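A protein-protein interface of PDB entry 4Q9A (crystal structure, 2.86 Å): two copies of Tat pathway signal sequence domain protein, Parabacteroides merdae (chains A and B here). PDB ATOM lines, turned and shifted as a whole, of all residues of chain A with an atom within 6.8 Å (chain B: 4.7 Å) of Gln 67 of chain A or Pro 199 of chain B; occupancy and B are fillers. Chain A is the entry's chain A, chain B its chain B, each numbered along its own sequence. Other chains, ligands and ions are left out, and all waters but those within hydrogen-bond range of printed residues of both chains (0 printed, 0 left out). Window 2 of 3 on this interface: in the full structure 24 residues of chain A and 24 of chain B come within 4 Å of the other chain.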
ATOM      1  N   LYS A  17      20.670  19.934  12.240  1.00  0.00           N
ATOM      2  CA  LYS A  17      22.075  19.782  12.612  1.00  0.00           C
ATOM      3  C   LYS A  17      22.864  19.265  11.410  1.00  0.00           C
ATOM      4  O   LYS A  17      22.261  18.926  10.397  1.00  0.00           O
ATOM      5  CB  LYS A  17      22.207  18.825  13.812  1.00  0.00           C
ATOM      6  CG  LYS A  17      21.649  17.416  13.581  1.00  0.00           C
ATOM      7  CD  LYS A  17      21.897  16.593  14.810  1.00  0.00           C
ATOM      8  CE  LYS A  17      21.286  15.234  14.751  1.00  0.00           C
ATOM      9  NZ  LYS A  17      21.294  14.593  16.097  1.00  0.00           N
ATOM     10  N   LYS A  18      24.204  19.174  11.520  1.00  0.00           N
ATOM     11  CA  LYS A  18      25.018  18.589  10.446  1.00  0.00           C
ATOM     12  C   LYS A  18      24.635  17.114  10.317  1.00  0.00           C
ATOM     13  O   LYS A  18      24.336  16.463  11.327  1.00  0.00           O
ATOM     14  CB  LYS A  18      26.536  18.756  10.693  1.00  0.00           C
ATOM     15  CG  LYS A  18      27.386  18.592   9.430  1.00  0.00           C
ATOM     16  CD  LYS A  18      28.889  18.786   9.679  1.00  0.00           C
ATOM     17  CE  LYS A  18      29.617  17.540  10.168  1.00  0.00           C
ATOM     18  NZ  LYS A  18      29.921  16.575   9.070  1.00  0.00           N
ATOM     19  N   ASP A  19      24.570  16.622   9.074  1.00  0.00           N
ATOM     20  CA  ASP A  19      24.241  15.240   8.719  1.00  0.00           C
ATOM     21  C   ASP A  19      22.877  14.802   9.319  1.00  0.00           C
ATOM     22  O   ASP A  19      22.691  13.624   9.626  1.00  0.00           O
ATOM     23  CB  ASP A  19      25.377  14.269   9.132  1.00  0.00           C
ATOM     24  CG  ASP A  19      26.775  14.751   8.789  1.00  0.00           C
ATOM     25  OD1 ASP A  19      27.035  15.027   7.596  1.00  0.00           O
ATOM     26  OD2 ASP A  19      27.621  14.823   9.708  1.00  0.00           O
ATOM     27  N   CYS A  20      21.921  15.737   9.438  1.00  0.00           N
ATOM     28  CA  CYS A  20      20.573  15.465   9.954  1.00  0.00           C
ATOM     29  C   CYS A  20      19.795  14.563   8.991  1.00  0.00           C
ATOM     30  O   CYS A  20      19.925  14.701   7.773  1.00  0.00           O
ATOM     31  CB  CYS A  20      19.811  16.764  10.211  1.00  0.00           C
ATOM     32  SG  CYS A  20      19.545  17.763   8.713  1.00  0.00           S
ATOM     33  N   ASN A  42      19.245  11.166  -1.003  1.00  0.00           N
ATOM     34  CA  ASN A  42      19.428  12.308  -1.890  1.00  0.00           C
ATOM     35  C   ASN A  42      19.571  11.973  -3.384  1.00  0.00           C
ATOM     36  O   ASN A  42      20.299  12.680  -4.089  1.00  0.00           O
ATOM     37  CB  ASN A  42      20.616  13.154  -1.399  1.00  0.00           C
ATOM     38  CG  ASN A  42      20.520  13.519   0.068  1.00  0.00           C
ATOM     39  OD1 ASN A  42      19.442  13.489   0.681  1.00  0.00           O
ATOM     40  ND2 ASN A  42      21.645  13.866   0.668  1.00  0.00           N
ATOM     41  N   LEU A  60      18.403  20.439   0.252  1.00  0.00           N
ATOM     42  CA  LEU A  60      19.751  20.085  -0.207  1.00  0.00           C
ATOM     43  C   LEU A  60      20.549  21.312  -0.683  1.00  0.00           C
ATOM     44  O   LEU A  60      21.756  21.354  -0.486  1.00  0.00           O
ATOM     45  CB  LEU A  60      19.687  19.049  -1.361  1.00  0.00           C
ATOM     46  CG  LEU A  60      19.235  17.630  -1.033  1.00  0.00           C
ATOM     47  CD1 LEU A  60      19.116  16.800  -2.287  1.00  0.00           C
ATOM     48  CD2 LEU A  60      20.184  16.964  -0.080  1.00  0.00           C
ATOM     49  N   LYS A  63      20.084  24.326   2.752  1.00  0.00           N
ATOM     50  CA  LYS A  63      20.781  23.931   3.973  1.00  0.00           C
ATOM     51  C   LYS A  63      21.975  23.007   3.649  1.00  0.00           C
ATOM     52  O   LYS A  63      22.285  22.079   4.409  1.00  0.00           O
ATOM     53  CB  LYS A  63      19.776  23.252   4.927  1.00  0.00           C
ATOM     54  CG  LYS A  63      18.497  24.050   5.234  1.00  0.00           C
ATOM     55  CD  LYS A  63      18.711  25.340   6.046  1.00  0.00           C
ATOM     56  CE  LYS A  63      17.392  26.050   6.290  1.00  0.00           C
ATOM     57  NZ  LYS A  63      17.573  27.486   6.633  1.00  0.00           N
ATOM     58  N   ALA A  64      22.664  23.283   2.521  1.00  0.00           N
ATOM     59  CA  ALA A  64      23.814  22.519   1.997  1.00  0.00           C
ATOM     60  C   ALA A  64      24.975  22.353   2.995  1.00  0.00           C
ATOM     61  O   ALA A  64      25.583  21.283   3.037  1.00  0.00           O
ATOM     62  CB  ALA A  64      24.333  23.178   0.742  1.00  0.00           C
ATOM     63  N   ALA A  65      25.274  23.408   3.795  1.00  0.00           N
ATOM     64  CA  ALA A  65      26.334  23.431   4.810  1.00  0.00           C
ATOM     65  C   ALA A  65      26.116  22.379   5.883  1.00  0.00           C
ATOM     66  O   ALA A  65      27.065  21.999   6.564  1.00  0.00           O
ATOM     67  CB  ALA A  65      26.395  24.799   5.452  1.00  0.00           C
ATOM     68  N   LEU A  66      24.873  21.895   6.020  1.00  0.00           N
ATOM     69  CA  LEU A  66      24.490  20.874   6.999  1.00  0.00           C
ATOM     70  C   LEU A  66      24.480  19.465   6.388  1.00  0.00           C
ATOM     71  O   LEU A  66      24.372  18.486   7.125  1.00  0.00           O
ATOM     72  CB  LEU A  66      23.114  21.211   7.587  1.00  0.00           C
ATOM     73  CG  LEU A  66      23.045  22.548   8.350  1.00  0.00           C
ATOM     74  CD1 LEU A  66      21.626  23.030   8.465  1.00  0.00           C
ATOM     75  CD2 LEU A  66      23.703  22.443   9.715  1.00  0.00           C
ATOM     76  N   GLN A  67      24.635  19.369   5.056  1.00  0.00           N
ATOM     77  CA  GLN A  67      24.647  18.126   4.267  1.00  0.00           C
ATOM     78  C   GLN A  67      23.580  17.132   4.785  1.00  0.00           C
ATOM     79  O   GLN A  67      23.917  16.103   5.381  1.00  0.00           O
ATOM     80  CB  GLN A  67      26.041  17.517   4.226  1.00  0.00           C
ATOM     81  CG  GLN A  67      26.926  18.237   3.225  1.00  0.00           C
ATOM     82  CD  GLN A  67      27.934  17.295   2.644  1.00  0.00           C
ATOM     83  OE1 GLN A  67      27.583  16.279   2.034  1.00  0.00           O
ATOM     84  NE2 GLN A  67      29.218  17.601   2.822  1.00  0.00           N
ATOM     85  N   PRO A  68      22.272  17.478   4.643  1.00  0.00           N
ATOM     86  CA  PRO A  68      21.228  16.590   5.169  1.00  0.00           C
ATOM     87  C   PRO A  68      21.056  15.308   4.349  1.00  0.00           C
ATOM     88  O   PRO A  68      21.330  15.292   3.138  1.00  0.00           O
ATOM     89  CB  PRO A  68      19.967  17.459   5.105  1.00  0.00           C
ATOM     90  CG  PRO A  68      20.220  18.453   4.072  1.00  0.00           C
ATOM     91  CD  PRO A  68      21.688  18.682   4.011  1.00  0.00           C
ATOM     92  N   LYS A  69      20.641  14.232   5.026  1.00  0.00           N
ATOM     93  CA  LYS A  69      20.383  12.943   4.386  1.00  0.00           C
ATOM     94  C   LYS A  69      18.871  12.800   4.339  1.00  0.00           C
ATOM     95  O   LYS A  69      18.236  12.654   5.394  1.00  0.00           O
ATOM     96  CB  LYS A  69      21.073  11.768   5.131  1.00  0.00           C
ATOM     97  CG  LYS A  69      22.492  12.043   5.671  1.00  0.00           C
ATOM     98  CD  LYS A  69      23.275  10.739   5.860  1.00  0.00           C
ATOM     99  CE  LYS A  69      24.288  10.826   6.962  1.00  0.00           C
ATOM    100  NZ  LYS A  69      24.984   9.539   7.173  1.00  0.00           N
ATOM    101  N   VAL B 195      30.495  26.030  -3.321  1.00  0.00           N
ATOM    102  CA  VAL B 195      31.613  25.167  -2.892  1.00  0.00           C
ATOM    103  C   VAL B 195      32.271  25.648  -1.585  1.00  0.00           C
ATOM    104  O   VAL B 195      33.047  24.895  -1.001  1.00  0.00           O
ATOM    105  CB  VAL B 195      32.696  24.924  -3.968  1.00  0.00           C
ATOM    106  CG1 VAL B 195      32.128  24.179  -5.170  1.00  0.00           C
ATOM    107  CG2 VAL B 195      33.394  26.217  -4.370  1.00  0.00           C
ATOM    108  N   ALA B 198      29.695  23.565   0.908  1.00  0.00           N
ATOM    109  CA  ALA B 198      29.778  22.100   0.777  1.00  0.00           C
ATOM    110  C   ALA B 198      30.722  21.729  -0.395  1.00  0.00           C
ATOM    111  O   ALA B 198      30.805  22.497  -1.360  1.00  0.00           O
ATOM    112  CB  ALA B 198      28.388  21.508   0.562  1.00  0.00           C
ATOM    113  N   PRO B 199      31.452  20.582  -0.341  1.00  0.00           N
ATOM    114  CA  PRO B 199      32.390  20.246  -1.444  1.00  0.00           C
ATOM    115  C   PRO B 199      31.729  20.133  -2.820  1.00  0.00           C
ATOM    116  O   PRO B 199      30.548  19.783  -2.939  1.00  0.00           O
ATOM    117  CB  PRO B 199      32.978  18.895  -1.025  1.00  0.00           C
ATOM    118  CG  PRO B 199      32.034  18.353   0.002  1.00  0.00           C
ATOM    119  CD  PRO B 199      31.494  19.556   0.724  1.00  0.00           C
ATOM    120  N   ALA B 200      32.523  20.422  -3.860  1.00  0.00           N
ATOM    121  CA  ALA B 200      32.119  20.422  -5.259  1.00  0.00           C
ATOM    122  C   ALA B 200      31.341  19.167  -5.648  1.00  0.00           C
ATOM    123  O   ALA B 200      30.321  19.310  -6.334  1.00  0.00           O
ATOM    124  CB  ALA B 200      33.339  20.586  -6.164  1.00  0.00           C
ATOM    125  N   ARG B 201      31.774  17.950  -5.167  1.00  0.00           N
ATOM    126  CA  ARG B 201      31.125  16.659  -5.513  1.00  0.00           C
ATOM    127  C   ARG B 201      29.674  16.577  -5.049  1.00  0.00           C
ATOM    128  O   ARG B 201      28.900  15.808  -5.635  1.00  0.00           O
ATOM    129  CB  ARG B 201      31.889  15.428  -5.018  1.00  0.00           C
ATOM    130  CG  ARG B 201      31.862  15.243  -3.523  1.00  0.00           C
ATOM    131  CD  ARG B 201      31.575  13.816  -3.094  1.00  0.00           C
ATOM    132  NE  ARG B 201      31.884  13.666  -1.671  1.00  0.00           N
ATOM    133  CZ  ARG B 201      31.046  13.940  -0.670  1.00  0.00           C
ATOM    134  NH1 ARG B 201      29.804  14.342  -0.923  1.00  0.00           N
ATOM    135  NH2 ARG B 201      31.437  13.796   0.588  1.00  0.00           N
ATOM    136  N   TYR B 202      29.308  17.380  -4.026  1.00  0.00           N
ATOM    137  CA  TYR B 202      27.956  17.443  -3.490  1.00  0.00           C
ATOM    138  C   TYR B 202      27.048  18.104  -4.543  1.00  0.00           C
ATOM    139  O   TYR B 202      25.930  17.640  -4.786  1.00  0.00           O
ATOM    140  CB  TYR B 202      27.950  18.218  -2.152  1.00  0.00           C
ATOM    141  CG  TYR B 202      26.570  18.448  -1.560  1.00  0.00           C
ATOM    142  CD1 TYR B 202      25.930  17.453  -0.826  1.00  0.00           C
ATOM    143  CD2 TYR B 202      25.914  19.666  -1.715  1.00  0.00           C
ATOM    144  CE1 TYR B 202      24.672  17.662  -0.267  1.00  0.00           C
ATOM    145  CE2 TYR B 202      24.663  19.890  -1.148  1.00  0.00           C
ATOM    146  CZ  TYR B 202      24.038  18.878  -0.438  1.00  0.00           C
ATOM    147  OH  TYR B 202      22.802  19.083   0.128  1.00  0.00           O
ATOM    148  N   TRP B 203      27.567  19.157  -5.188  1.00  0.00           N
ATOM    149  CA  TRP B 203      26.860  19.946  -6.187  1.00  0.00           C
ATOM    150  C   TRP B 203      26.874  19.280  -7.552  1.00  0.00           C
ATOM    151  O   TRP B 203      25.866  19.329  -8.266  1.00  0.00           O
ATOM    152  CB  TRP B 203      27.496  21.333  -6.289  1.00  0.00           C
ATOM    153  CG  TRP B 203      27.532  22.057  -4.977  1.00  0.00           C
ATOM    154  CD1 TRP B 203      28.590  22.155  -4.119  1.00  0.00           C
ATOM    155  CD2 TRP B 203      26.428  22.715  -4.336  1.00  0.00           C
ATOM    156  NE1 TRP B 203      28.228  22.876  -3.006  1.00  0.00           N
ATOM    157  CE2 TRP B 203      26.904  23.223  -3.107  1.00  0.00           C
ATOM    158  CE3 TRP B 203      25.078  22.935  -4.694  1.00  0.00           C
ATOM    159  CZ2 TRP B 203      26.081  23.931  -2.230  1.00  0.00           C
ATOM    160  CZ3 TRP B 203      24.266  23.658  -3.835  1.00  0.00           C
ATOM    161  CH2 TRP B 203      24.763  24.140  -2.616  1.00  0.00           C
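Ala 64 of chain A touches Ala 198 of chain B (O to CB, 3.7 Å). Ala 64 of chain A touches Tyr 202 of chain B. Trp 203 of chain B touches Ala 64 of chain A. Gln 67 of chain A touches Pro 199 of chain B (NE2 to CD, 3.7 Å). Gln 67 of chain A touches Tyr 202 of chain B (OE1 to CD1, 3.5 Å).
Of the 7 printed residues of chain B, 4 touch a printed residue of chain A. Printed residues of chain B that touch a printed residue of chain A: Ala 198, Pro 199, Tyr 202 and Trp 203. Hydrophobic or aromatic side chains of chain B within 4 Å of the printed part of chain A: Ala 198, Pro 199, Tyr 202 and Trp 203. Among the printed residues, 6 pairs touch across the chains. Among the printed residues, no Asp or Glu carboxylate lies within 4 Å of a Lys or Arg side-chain nitrogen of the other chain.
The backbone carbonyl oxygen (O) of Leu 60 of chain A is in hydrogen-bond range of the side-chain hydroxyl (OH) of Tyr 202 of chain B (2.6 Å).
No position is printed for both chains.
Of chain A, only Gln 67 (3.7 Å) comes within 4 Å of Pro 199 of chain B. Printed residues of chain B within 4 Å of Leu 60 of chain A: Tyr 202 (2.6 Å). Of the printed residues of chain B, Ala 64 of chain A touches Ala 198, Tyr 202 and Trp 203. Of the printed residues of chain A, Trp 203 of chain B touches Ala 64 (3.5 Å). Asn 42 of chain A touches none of the printed residues of chain B. Ala 65 of chain A touches none of the printed residues of chain B. The nearest residue of chain A that does not touch Pro 199 of chain B is Ala 64 of chain A (6.6 Å).
The indole nitrogen (NE1) of Trp 203 of chain B lies within hydrogen-bond range of the backbone carbonyl oxygen (O) of Ala 198 of chain B (3.1 Å).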
